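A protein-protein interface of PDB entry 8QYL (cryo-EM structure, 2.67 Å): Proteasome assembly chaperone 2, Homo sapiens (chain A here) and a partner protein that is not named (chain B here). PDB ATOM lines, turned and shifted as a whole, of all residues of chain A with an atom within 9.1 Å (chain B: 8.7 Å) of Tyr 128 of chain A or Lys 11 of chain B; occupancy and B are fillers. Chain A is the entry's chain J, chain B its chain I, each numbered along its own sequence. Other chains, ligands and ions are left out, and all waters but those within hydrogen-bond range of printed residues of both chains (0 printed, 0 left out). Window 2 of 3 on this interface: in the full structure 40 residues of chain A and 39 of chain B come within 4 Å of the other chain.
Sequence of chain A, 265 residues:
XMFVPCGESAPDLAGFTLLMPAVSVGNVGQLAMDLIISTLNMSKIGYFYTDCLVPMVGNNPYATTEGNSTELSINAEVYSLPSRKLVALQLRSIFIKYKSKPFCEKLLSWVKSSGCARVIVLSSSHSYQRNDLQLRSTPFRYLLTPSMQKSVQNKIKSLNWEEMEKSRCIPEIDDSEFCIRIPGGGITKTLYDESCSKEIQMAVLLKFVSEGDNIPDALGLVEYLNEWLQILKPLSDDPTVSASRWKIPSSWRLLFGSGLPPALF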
ATOM      1  N   VAL A  25     -18.155  21.185  21.832  1.00  0.00           N
ATOM      2  CA  VAL A  25     -19.235  20.989  22.791  1.00  0.00           C
ATOM      3  C   VAL A  25     -18.773  21.403  24.181  1.00  0.00           C
ATOM      4  O   VAL A  25     -17.717  20.973  24.662  1.00  0.00           O
ATOM      5  CB  VAL A  25     -19.722  19.531  22.760  1.00  0.00           C
ATOM      6  CG1 VAL A  25     -18.572  18.564  22.977  1.00  0.00           C
ATOM      7  CG2 VAL A  25     -20.799  19.310  23.803  1.00  0.00           C
ATOM      8  N   SER A 125     -15.164  16.186  22.911  1.00  0.00           N
ATOM      9  CA  SER A 125     -16.012  15.322  22.105  1.00  0.00           C
ATOM     10  C   SER A 125     -17.201  14.851  22.930  1.00  0.00           C
ATOM     11  O   SER A 125     -17.168  14.852  24.162  1.00  0.00           O
ATOM     12  CB  SER A 125     -15.231  14.119  21.564  1.00  0.00           C
ATOM     13  OG  SER A 125     -15.937  13.491  20.512  1.00  0.00           O
ATOM     14  N   HIS A 126     -18.254  14.438  22.226  1.00  0.00           N
ATOM     15  CA  HIS A 126     -19.486  14.008  22.877  1.00  0.00           C
ATOM     16  C   HIS A 126     -19.249  12.784  23.750  1.00  0.00           C
ATOM     17  O   HIS A 126     -18.559  11.841  23.357  1.00  0.00           O
ATOM     18  CB  HIS A 126     -20.555  13.696  21.833  1.00  0.00           C
ATOM     19  CG  HIS A 126     -21.245  14.906  21.292  1.00  0.00           C
ATOM     20  ND1 HIS A 126     -21.526  15.066  19.954  1.00  0.00           N
ATOM     21  CD2 HIS A 126     -21.716  16.013  21.910  1.00  0.00           C
ATOM     22  CE1 HIS A 126     -22.138  16.221  19.770  1.00  0.00           C
ATOM     23  NE2 HIS A 126     -22.264  16.816  20.941  1.00  0.00           N
ATOM     24  N   SER A 127     -19.839  12.800  24.942  1.00  0.00           N
ATOM     25  CA  SER A 127     -19.660  11.732  25.914  1.00  0.00           C
ATOM     26  C   SER A 127     -20.690  10.620  25.788  1.00  0.00           C
ATOM     27  O   SER A 127     -20.540   9.586  26.444  1.00  0.00           O
ATOM     28  CB  SER A 127     -19.709  12.302  27.333  1.00  0.00           C
ATOM     29  OG  SER A 127     -19.492  11.292  28.298  1.00  0.00           O
ATOM     30  N   TYR A 128     -21.723  10.795  24.970  1.00  0.00           N
ATOM     31  CA  TYR A 128     -22.736   9.765  24.803  1.00  0.00           C
ATOM     32  C   TYR A 128     -22.418   8.802  23.666  1.00  0.00           C
ATOM     33  O   TYR A 128     -23.208   7.891  23.408  1.00  0.00           O
ATOM     34  CB  TYR A 128     -24.117  10.402  24.591  1.00  0.00           C
ATOM     35  CG  TYR A 128     -24.349  11.020  23.230  1.00  0.00           C
ATOM     36  CD1 TYR A 128     -24.033  12.348  22.989  1.00  0.00           C
ATOM     37  CD2 TYR A 128     -24.904  10.283  22.195  1.00  0.00           C
ATOM     38  CE1 TYR A 128     -24.251  12.919  21.754  1.00  0.00           C
ATOM     39  CE2 TYR A 128     -25.121  10.845  20.957  1.00  0.00           C
ATOM     40  CZ  TYR A 128     -24.792  12.162  20.742  1.00  0.00           C
ATOM     41  OH  TYR A 128     -25.010  12.728  19.510  1.00  0.00           O
ATOM     42  N   GLN A 129     -21.280   8.971  22.995  1.00  0.00           N
ATOM     43  CA  GLN A 129     -20.854   8.075  21.929  1.00  0.00           C
ATOM     44  C   GLN A 129     -19.673   7.207  22.352  1.00  0.00           C
ATOM     45  O   GLN A 129     -18.839   6.837  21.525  1.00  0.00           O
ATOM     46  CB  GLN A 129     -20.507   8.868  20.672  1.00  0.00           C
ATOM     47  CG  GLN A 129     -21.556   9.885  20.288  1.00  0.00           C
ATOM     48  CD  GLN A 129     -21.487  10.262  18.827  1.00  0.00           C
ATOM     49  OE1 GLN A 129     -20.669   9.732  18.077  1.00  0.00           O
ATOM     50  NE2 GLN A 129     -22.350  11.179  18.411  1.00  0.00           N
ATOM     51  N   ARG A 130     -19.591   6.879  23.635  1.00  0.00           N
ATOM     52  CA  ARG A 130     -18.563   5.998  24.163  1.00  0.00           C
ATOM     53  C   ARG A 130     -19.081   4.568  24.217  1.00  0.00           C
ATOM     54  O   ARG A 130     -20.269   4.329  24.445  1.00  0.00           O
ATOM     55  CB  ARG A 130     -18.131   6.443  25.560  1.00  0.00           C
ATOM     56  CG  ARG A 130     -17.056   7.502  25.576  1.00  0.00           C
ATOM     57  CD  ARG A 130     -16.611   7.793  26.992  1.00  0.00           C
ATOM     58  NE  ARG A 130     -17.750   8.022  27.870  1.00  0.00           N
ATOM     59  CZ  ARG A 130     -17.658   8.281  29.166  1.00  0.00           C
ATOM     60  NH1 ARG A 130     -16.485   8.365  29.772  1.00  0.00           N
ATOM     61  NH2 ARG A 130     -18.770   8.460  29.873  1.00  0.00           N
ATOM     62  N   ASN A 131     -18.178   3.614  24.002  1.00  0.00           N
ATOM     63  CA  ASN A 131     -18.530   2.205  24.086  1.00  0.00           C
ATOM     64  C   ASN A 131     -18.206   1.682  25.484  1.00  0.00           C
ATOM     65  O   ASN A 131     -17.838   2.437  26.387  1.00  0.00           O
ATOM     66  CB  ASN A 131     -17.826   1.411  22.987  1.00  0.00           C
ATOM     67  CG  ASN A 131     -16.317   1.581  23.007  1.00  0.00           C
ATOM     68  OD1 ASN A 131     -15.736   1.982  24.010  1.00  0.00           O
ATOM     69  ND2 ASN A 131     -15.677   1.264  21.890  1.00  0.00           N
ATOM     70  N   GLN A 134     -14.482   2.221  26.480  1.00  0.00           N
ATOM     71  CA  GLN A 134     -14.211   3.618  26.797  1.00  0.00           C
ATOM     72  C   GLN A 134     -14.918   4.055  28.072  1.00  0.00           C
ATOM     73  O   GLN A 134     -14.470   4.998  28.733  1.00  0.00           O
ATOM     74  CB  GLN A 134     -14.629   4.512  25.631  1.00  0.00           C
ATOM     75  CG  GLN A 134     -13.590   4.637  24.536  1.00  0.00           C
ATOM     76  CD  GLN A 134     -14.183   5.100  23.225  1.00  0.00           C
ATOM     77  OE1 GLN A 134     -15.393   5.051  23.028  1.00  0.00           O
ATOM     78  NE2 GLN A 134     -13.330   5.556  22.319  1.00  0.00           N
ATOM     79  N   LEU A 135     -16.019   3.392  28.430  1.00  0.00           N
ATOM     80  CA  LEU A 135     -16.767   3.761  29.625  1.00  0.00           C
ATOM     81  C   LEU A 135     -15.993   3.491  30.908  1.00  0.00           C
ATOM     82  O   LEU A 135     -16.309   4.089  31.941  1.00  0.00           O
ATOM     83  CB  LEU A 135     -18.098   3.012  29.663  1.00  0.00           C
ATOM     84  CG  LEU A 135     -19.319   3.766  29.144  1.00  0.00           C
ATOM     85  CD1 LEU A 135     -20.578   2.944  29.329  1.00  0.00           C
ATOM     86  CD2 LEU A 135     -19.445   5.098  29.850  1.00  0.00           C
ATOM     87  N   PRO A 183     -16.688  13.443  16.973  1.00  0.00           N
ATOM     88  CA  PRO A 183     -18.046  14.010  17.000  1.00  0.00           C
ATOM     89  C   PRO A 183     -18.158  15.101  18.055  1.00  0.00           C
ATOM     90  O   PRO A 183     -17.880  14.874  19.234  1.00  0.00           O
ATOM     91  CB  PRO A 183     -18.929  12.804  17.333  1.00  0.00           C
ATOM     92  CG  PRO A 183     -18.016  11.824  17.986  1.00  0.00           C
ATOM     93  CD  PRO A 183     -16.667  12.025  17.371  1.00  0.00           C
ATOM     94  N   GLY A 184     -18.583  16.285  17.625  1.00  0.00           N
ATOM     95  CA  GLY A 184     -18.670  17.425  18.511  1.00  0.00           C
ATOM     96  C   GLY A 184     -17.389  18.207  18.674  1.00  0.00           C
ATOM     97  O   GLY A 184     -17.264  18.960  19.645  1.00  0.00           O
ATOM     98  N   PHE A 208     -13.871  13.850  26.910  1.00  0.00           N
ATOM     99  CA  PHE A 208     -15.273  13.496  26.727  1.00  0.00           C
ATOM    100  C   PHE A 208     -16.120  14.229  27.761  1.00  0.00           C
ATOM    101  O   PHE A 208     -15.946  14.026  28.966  1.00  0.00           O
ATOM    102  CB  PHE A 208     -15.461  11.986  26.856  1.00  0.00           C
ATOM    103  CG  PHE A 208     -14.938  11.203  25.688  1.00  0.00           C
ATOM    104  CD1 PHE A 208     -15.666  11.114  24.516  1.00  0.00           C
ATOM    105  CD2 PHE A 208     -13.724  10.546  25.765  1.00  0.00           C
ATOM    106  CE1 PHE A 208     -15.191  10.392  23.444  1.00  0.00           C
ATOM    107  CE2 PHE A 208     -13.243   9.823  24.694  1.00  0.00           C
ATOM    108  CZ  PHE A 208     -13.978   9.747  23.533  1.00  0.00           C
ATOM    109  N   VAL A 209     -17.038  15.080  27.296  1.00  0.00           N
ATOM    110  CA  VAL A 209     -17.806  15.949  28.178  1.00  0.00           C
ATOM    111  C   VAL A 209     -19.271  15.963  27.766  1.00  0.00           C
ATOM    112  O   VAL A 209     -19.634  15.590  26.650  1.00  0.00           O
ATOM    113  CB  VAL A 209     -17.264  17.396  28.192  1.00  0.00           C
ATOM    114  CG1 VAL A 209     -15.866  17.441  28.782  1.00  0.00           C
ATOM    115  CG2 VAL A 209     -17.289  17.981  26.795  1.00  0.00           C
ATOM    116  N   SER A 210     -20.109  16.413  28.693  1.00  0.00           N
ATOM    117  CA  SER A 210     -21.521  16.662  28.454  1.00  0.00           C
ATOM    118  C   SER A 210     -21.838  18.100  28.840  1.00  0.00           C
ATOM    119  O   SER A 210     -21.208  18.669  29.736  1.00  0.00           O
ATOM    120  CB  SER A 210     -22.402  15.693  29.241  1.00  0.00           C
ATOM    121  OG  SER A 210     -23.707  15.639  28.698  1.00  0.00           O
ATOM    122  N   GLU A 211     -22.816  18.686  28.161  1.00  0.00           N
ATOM    123  CA  GLU A 211     -23.043  20.122  28.241  1.00  0.00           C
ATOM    124  C   GLU A 211     -23.804  20.506  29.506  1.00  0.00           C
ATOM    125  O   GLU A 211     -24.792  19.866  29.877  1.00  0.00           O
ATOM    126  CB  GLU A 211     -23.800  20.592  27.003  1.00  0.00           C
ATOM    127  CG  GLU A 211     -24.243  22.032  27.039  1.00  0.00           C
ATOM    128  CD  GLU A 211     -24.616  22.544  25.668  1.00  0.00           C
ATOM    129  OE1 GLU A 211     -23.821  22.354  24.725  1.00  0.00           O
ATOM    130  OE2 GLU A 211     -25.711  23.125  25.532  1.00  0.00           O
ATOM    131  N   ALA B   3     -39.887  14.989  21.344  1.00  0.00           N
ATOM    132  CA  ALA B   3     -40.485  13.661  21.333  1.00  0.00           C
ATOM    133  C   ALA B   3     -41.862  13.687  20.680  1.00  0.00           C
ATOM    134  O   ALA B   3     -42.801  14.272  21.213  1.00  0.00           O
ATOM    135  CB  ALA B   3     -40.581  13.114  22.743  1.00  0.00           C
ATOM    136  N   GLU B   8     -39.417   8.087  22.601  1.00  0.00           N
ATOM    137  CA  GLU B   8     -38.591   8.438  21.456  1.00  0.00           C
ATOM    138  C   GLU B   8     -37.256   8.992  21.934  1.00  0.00           C
ATOM    139  O   GLU B   8     -37.217   9.844  22.826  1.00  0.00           O
ATOM    140  CB  GLU B   8     -39.293   9.460  20.563  1.00  0.00           C
ATOM    141  CG  GLU B   8     -38.454   9.905  19.385  1.00  0.00           C
ATOM    142  CD  GLU B   8     -39.112  10.991  18.572  1.00  0.00           C
ATOM    143  OE1 GLU B   8     -40.234  11.401  18.926  1.00  0.00           O
ATOM    144  OE2 GLU B   8     -38.510  11.435  17.574  1.00  0.00           O
ATOM    145  N   VAL B   9     -36.170   8.506  21.342  1.00  0.00           N
ATOM    146  CA  VAL B   9     -34.829   8.949  21.708  1.00  0.00           C
ATOM    147  C   VAL B   9     -34.558  10.298  21.059  1.00  0.00           C
ATOM    148  O   VAL B   9     -34.762  10.471  19.852  1.00  0.00           O
ATOM    149  CB  VAL B   9     -33.780   7.906  21.290  1.00  0.00           C
ATOM    150  CG1 VAL B   9     -32.382   8.411  21.587  1.00  0.00           C
ATOM    151  CG2 VAL B   9     -34.034   6.587  21.999  1.00  0.00           C
ATOM    152  N   VAL B  10     -34.100  11.260  21.858  1.00  0.00           N
ATOM    153  CA  VAL B  10     -33.828  12.609  21.384  1.00  0.00           C
ATOM    154  C   VAL B  10     -32.425  13.014  21.812  1.00  0.00           C
ATOM    155  O   VAL B  10     -31.851  12.462  22.752  1.00  0.00           O
ATOM    156  CB  VAL B  10     -34.864  13.633  21.899  1.00  0.00           C
ATOM    157  CG1 VAL B  10     -36.241  13.324  21.341  1.00  0.00           C
ATOM    158  CG2 VAL B  10     -34.892  13.646  23.415  1.00  0.00           C
ATOM    159  N   LYS B  11     -31.878  14.000  21.109  1.00  0.00           N
ATOM    160  CA  LYS B  11     -30.540  14.509  21.368  1.00  0.00           C
ATOM    161  C   LYS B  11     -30.615  15.935  21.896  1.00  0.00           C
ATOM    162  O   LYS B  11     -31.459  16.725  21.463  1.00  0.00           O
ATOM    163  CB  LYS B  11     -29.679  14.462  20.103  1.00  0.00           C
ATOM    164  CG  LYS B  11     -29.195  13.069  19.744  1.00  0.00           C
ATOM    165  CD  LYS B  11     -28.751  12.988  18.296  1.00  0.00           C
ATOM    166  CE  LYS B  11     -28.255  11.591  17.947  1.00  0.00           C
ATOM    167  NZ  LYS B  11     -29.294  10.549  18.178  1.00  0.00           N
ATOM    168  N   ALA B  12     -29.730  16.254  22.836  1.00  0.00           N
ATOM    169  CA  ALA B  12     -29.734  17.565  23.461  1.00  0.00           C
ATOM    170  C   ALA B  12     -29.209  18.628  22.494  1.00  0.00           C
ATOM    171  O   ALA B  12     -28.422  18.326  21.592  1.00  0.00           O
ATOM    172  CB  ALA B  12     -28.885  17.549  24.727  1.00  0.00           C
ATOM    173  N   PRO B  13     -29.635  19.879  22.656  1.00  0.00           N
ATOM    174  CA  PRO B  13     -29.106  20.960  21.815  1.00  0.00           C
ATOM    175  C   PRO B  13     -27.690  21.341  22.225  1.00  0.00           C
ATOM    176  O   PRO B  13     -27.187  20.955  23.281  1.00  0.00           O
ATOM    177  CB  PRO B  13     -30.089  22.108  22.053  1.00  0.00           C
ATOM    178  CG  PRO B  13     -30.653  21.839  23.406  1.00  0.00           C
ATOM    179  CD  PRO B  13     -30.715  20.346  23.543  1.00  0.00           C
ATOM    180  N   CYS B  14     -27.041  22.118  21.361  1.00  0.00           N
ATOM    181  CA  CYS B  14     -25.646  22.500  21.537  1.00  0.00           C
ATOM    182  C   CYS B  14     -25.510  24.017  21.516  1.00  0.00           C
ATOM    183  O   CYS B  14     -26.030  24.678  20.613  1.00  0.00           O
ATOM    184  CB  CYS B  14     -24.770  21.874  20.449  1.00  0.00           C
ATOM    185  SG  CYS B  14     -22.994  22.074  20.706  1.00  0.00           S
ATOM    186  N   THR B  18     -22.312  23.046  16.934  1.00  0.00           N
ATOM    187  CA  THR B  18     -21.551  21.996  16.256  1.00  0.00           C
ATOM    188  C   THR B  18     -22.496  20.850  15.893  1.00  0.00           C
ATOM    189  O   THR B  18     -22.438  19.743  16.432  1.00  0.00           O
ATOM    190  CB  THR B  18     -20.401  21.517  17.131  1.00  0.00           C
ATOM    191  OG1 THR B  18     -20.917  21.012  18.368  1.00  0.00           O
ATOM    192  CG2 THR B  18     -19.444  22.658  17.422  1.00  0.00           C
ATOM    193  N   GLU B  22     -20.084  19.614  10.899  1.00  0.00           N
ATOM    194  CA  GLU B  22     -19.346  18.356  10.890  1.00  0.00           C
ATOM    195  C   GLU B  22     -19.919  17.367   9.883  1.00  0.00           C
ATOM    196  O   GLU B  22     -19.167  16.605   9.264  1.00  0.00           O
ATOM    197  CB  GLU B  22     -19.341  17.752  12.293  1.00  0.00           C
ATOM    198  CG  GLU B  22     -18.668  18.637  13.325  1.00  0.00           C
ATOM    199  CD  GLU B  22     -18.825  18.114  14.734  1.00  0.00           C
ATOM    200  OE1 GLU B  22     -19.530  17.102  14.925  1.00  0.00           O
ATOM    201  OE2 GLU B  22     -18.247  18.726  15.655  1.00  0.00           O
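Among the printed residues, pairs that only touch across the chains: Tyr 128 of chain A with Lys 11 of chain B (3.8 Å), Pro 183 of chain A with Glu 22 of chain B (3.96 Å) and Glu 211 of chain A with Cys 14 of chain B (3.7 Å).
The backbone NH (N) of Val 25 of chain A lies within hydrogen-bond range of the backbone carbonyl oxygen (O) of Gly 184 of chain A, at 3.2 Å.
The side-chain hydroxyl (OG) of Ser 125 of chain A sits at hydrogen-bond distance from the backbone carbonyl oxygen (O) of Pro 183 of chain A.
N of His 126 of chain A is in hydrogen-bond range of O of Pro 183 of chain A.
The side-chain hydroxyl (OH) of Tyr 128 of chain A sits at hydrogen-bond distance from the side-chain amide nitrogen (NE2) of Gln 129 of chain A.
The side-chain hydroxyl (OG1) of Thr 18 of chain B lies within hydrogen-bond range of the side-chain sulfur (SG) of Cys 14 of chain B, 3.3 Å away.
The side-chain carboxylate of Glu 22 of chain B is in hydrogen-bond range of the backbone NH of Gly 184 of chain A (3.0 Å).
OE2 of Glu 211 of chain A lies close to O of Pro 13 of chain B, 3.5 Å away.
Along chain B the printed residues that touch a printed residue of chain A span positions 11 to 22.
Of the 16 printed residues of chain A, 4 touch a printed residue of chain B.
Val 25 of chain A touches none of the printed residues of chain B.
No residue of chain B comes within 4 Å of Ser 127 of chain A.
Of chain B, only Lys 11 comes within 4 Å of Tyr 128 of chain A.
Leu 135 of chain A touches none of the printed residues of chain B.
Of the printed residues of chain B, Pro 183 of chain A touches Glu 22.
Of the printed residues of chain B, Glu 211 of chain A touches Pro 13 and Cys 14.
No residue of chain A comes within 4 Å of Val 10 of chain B.
Of chain A, only Tyr 128 comes within 4 Å of Lys 11 of chain B.
No residue of chain A comes within 4 Å of Ala 12 of chain B.
Of the printed residues of chain A, Pro 13 of chain B touches Glu 211.
Printed residues of chain A within 4 Å of Cys 14 of chain B: Glu 211 (3.7 Å).
Of the printed residues of chain A, Glu 22 of chain B touches Pro 183 and Gly 184.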
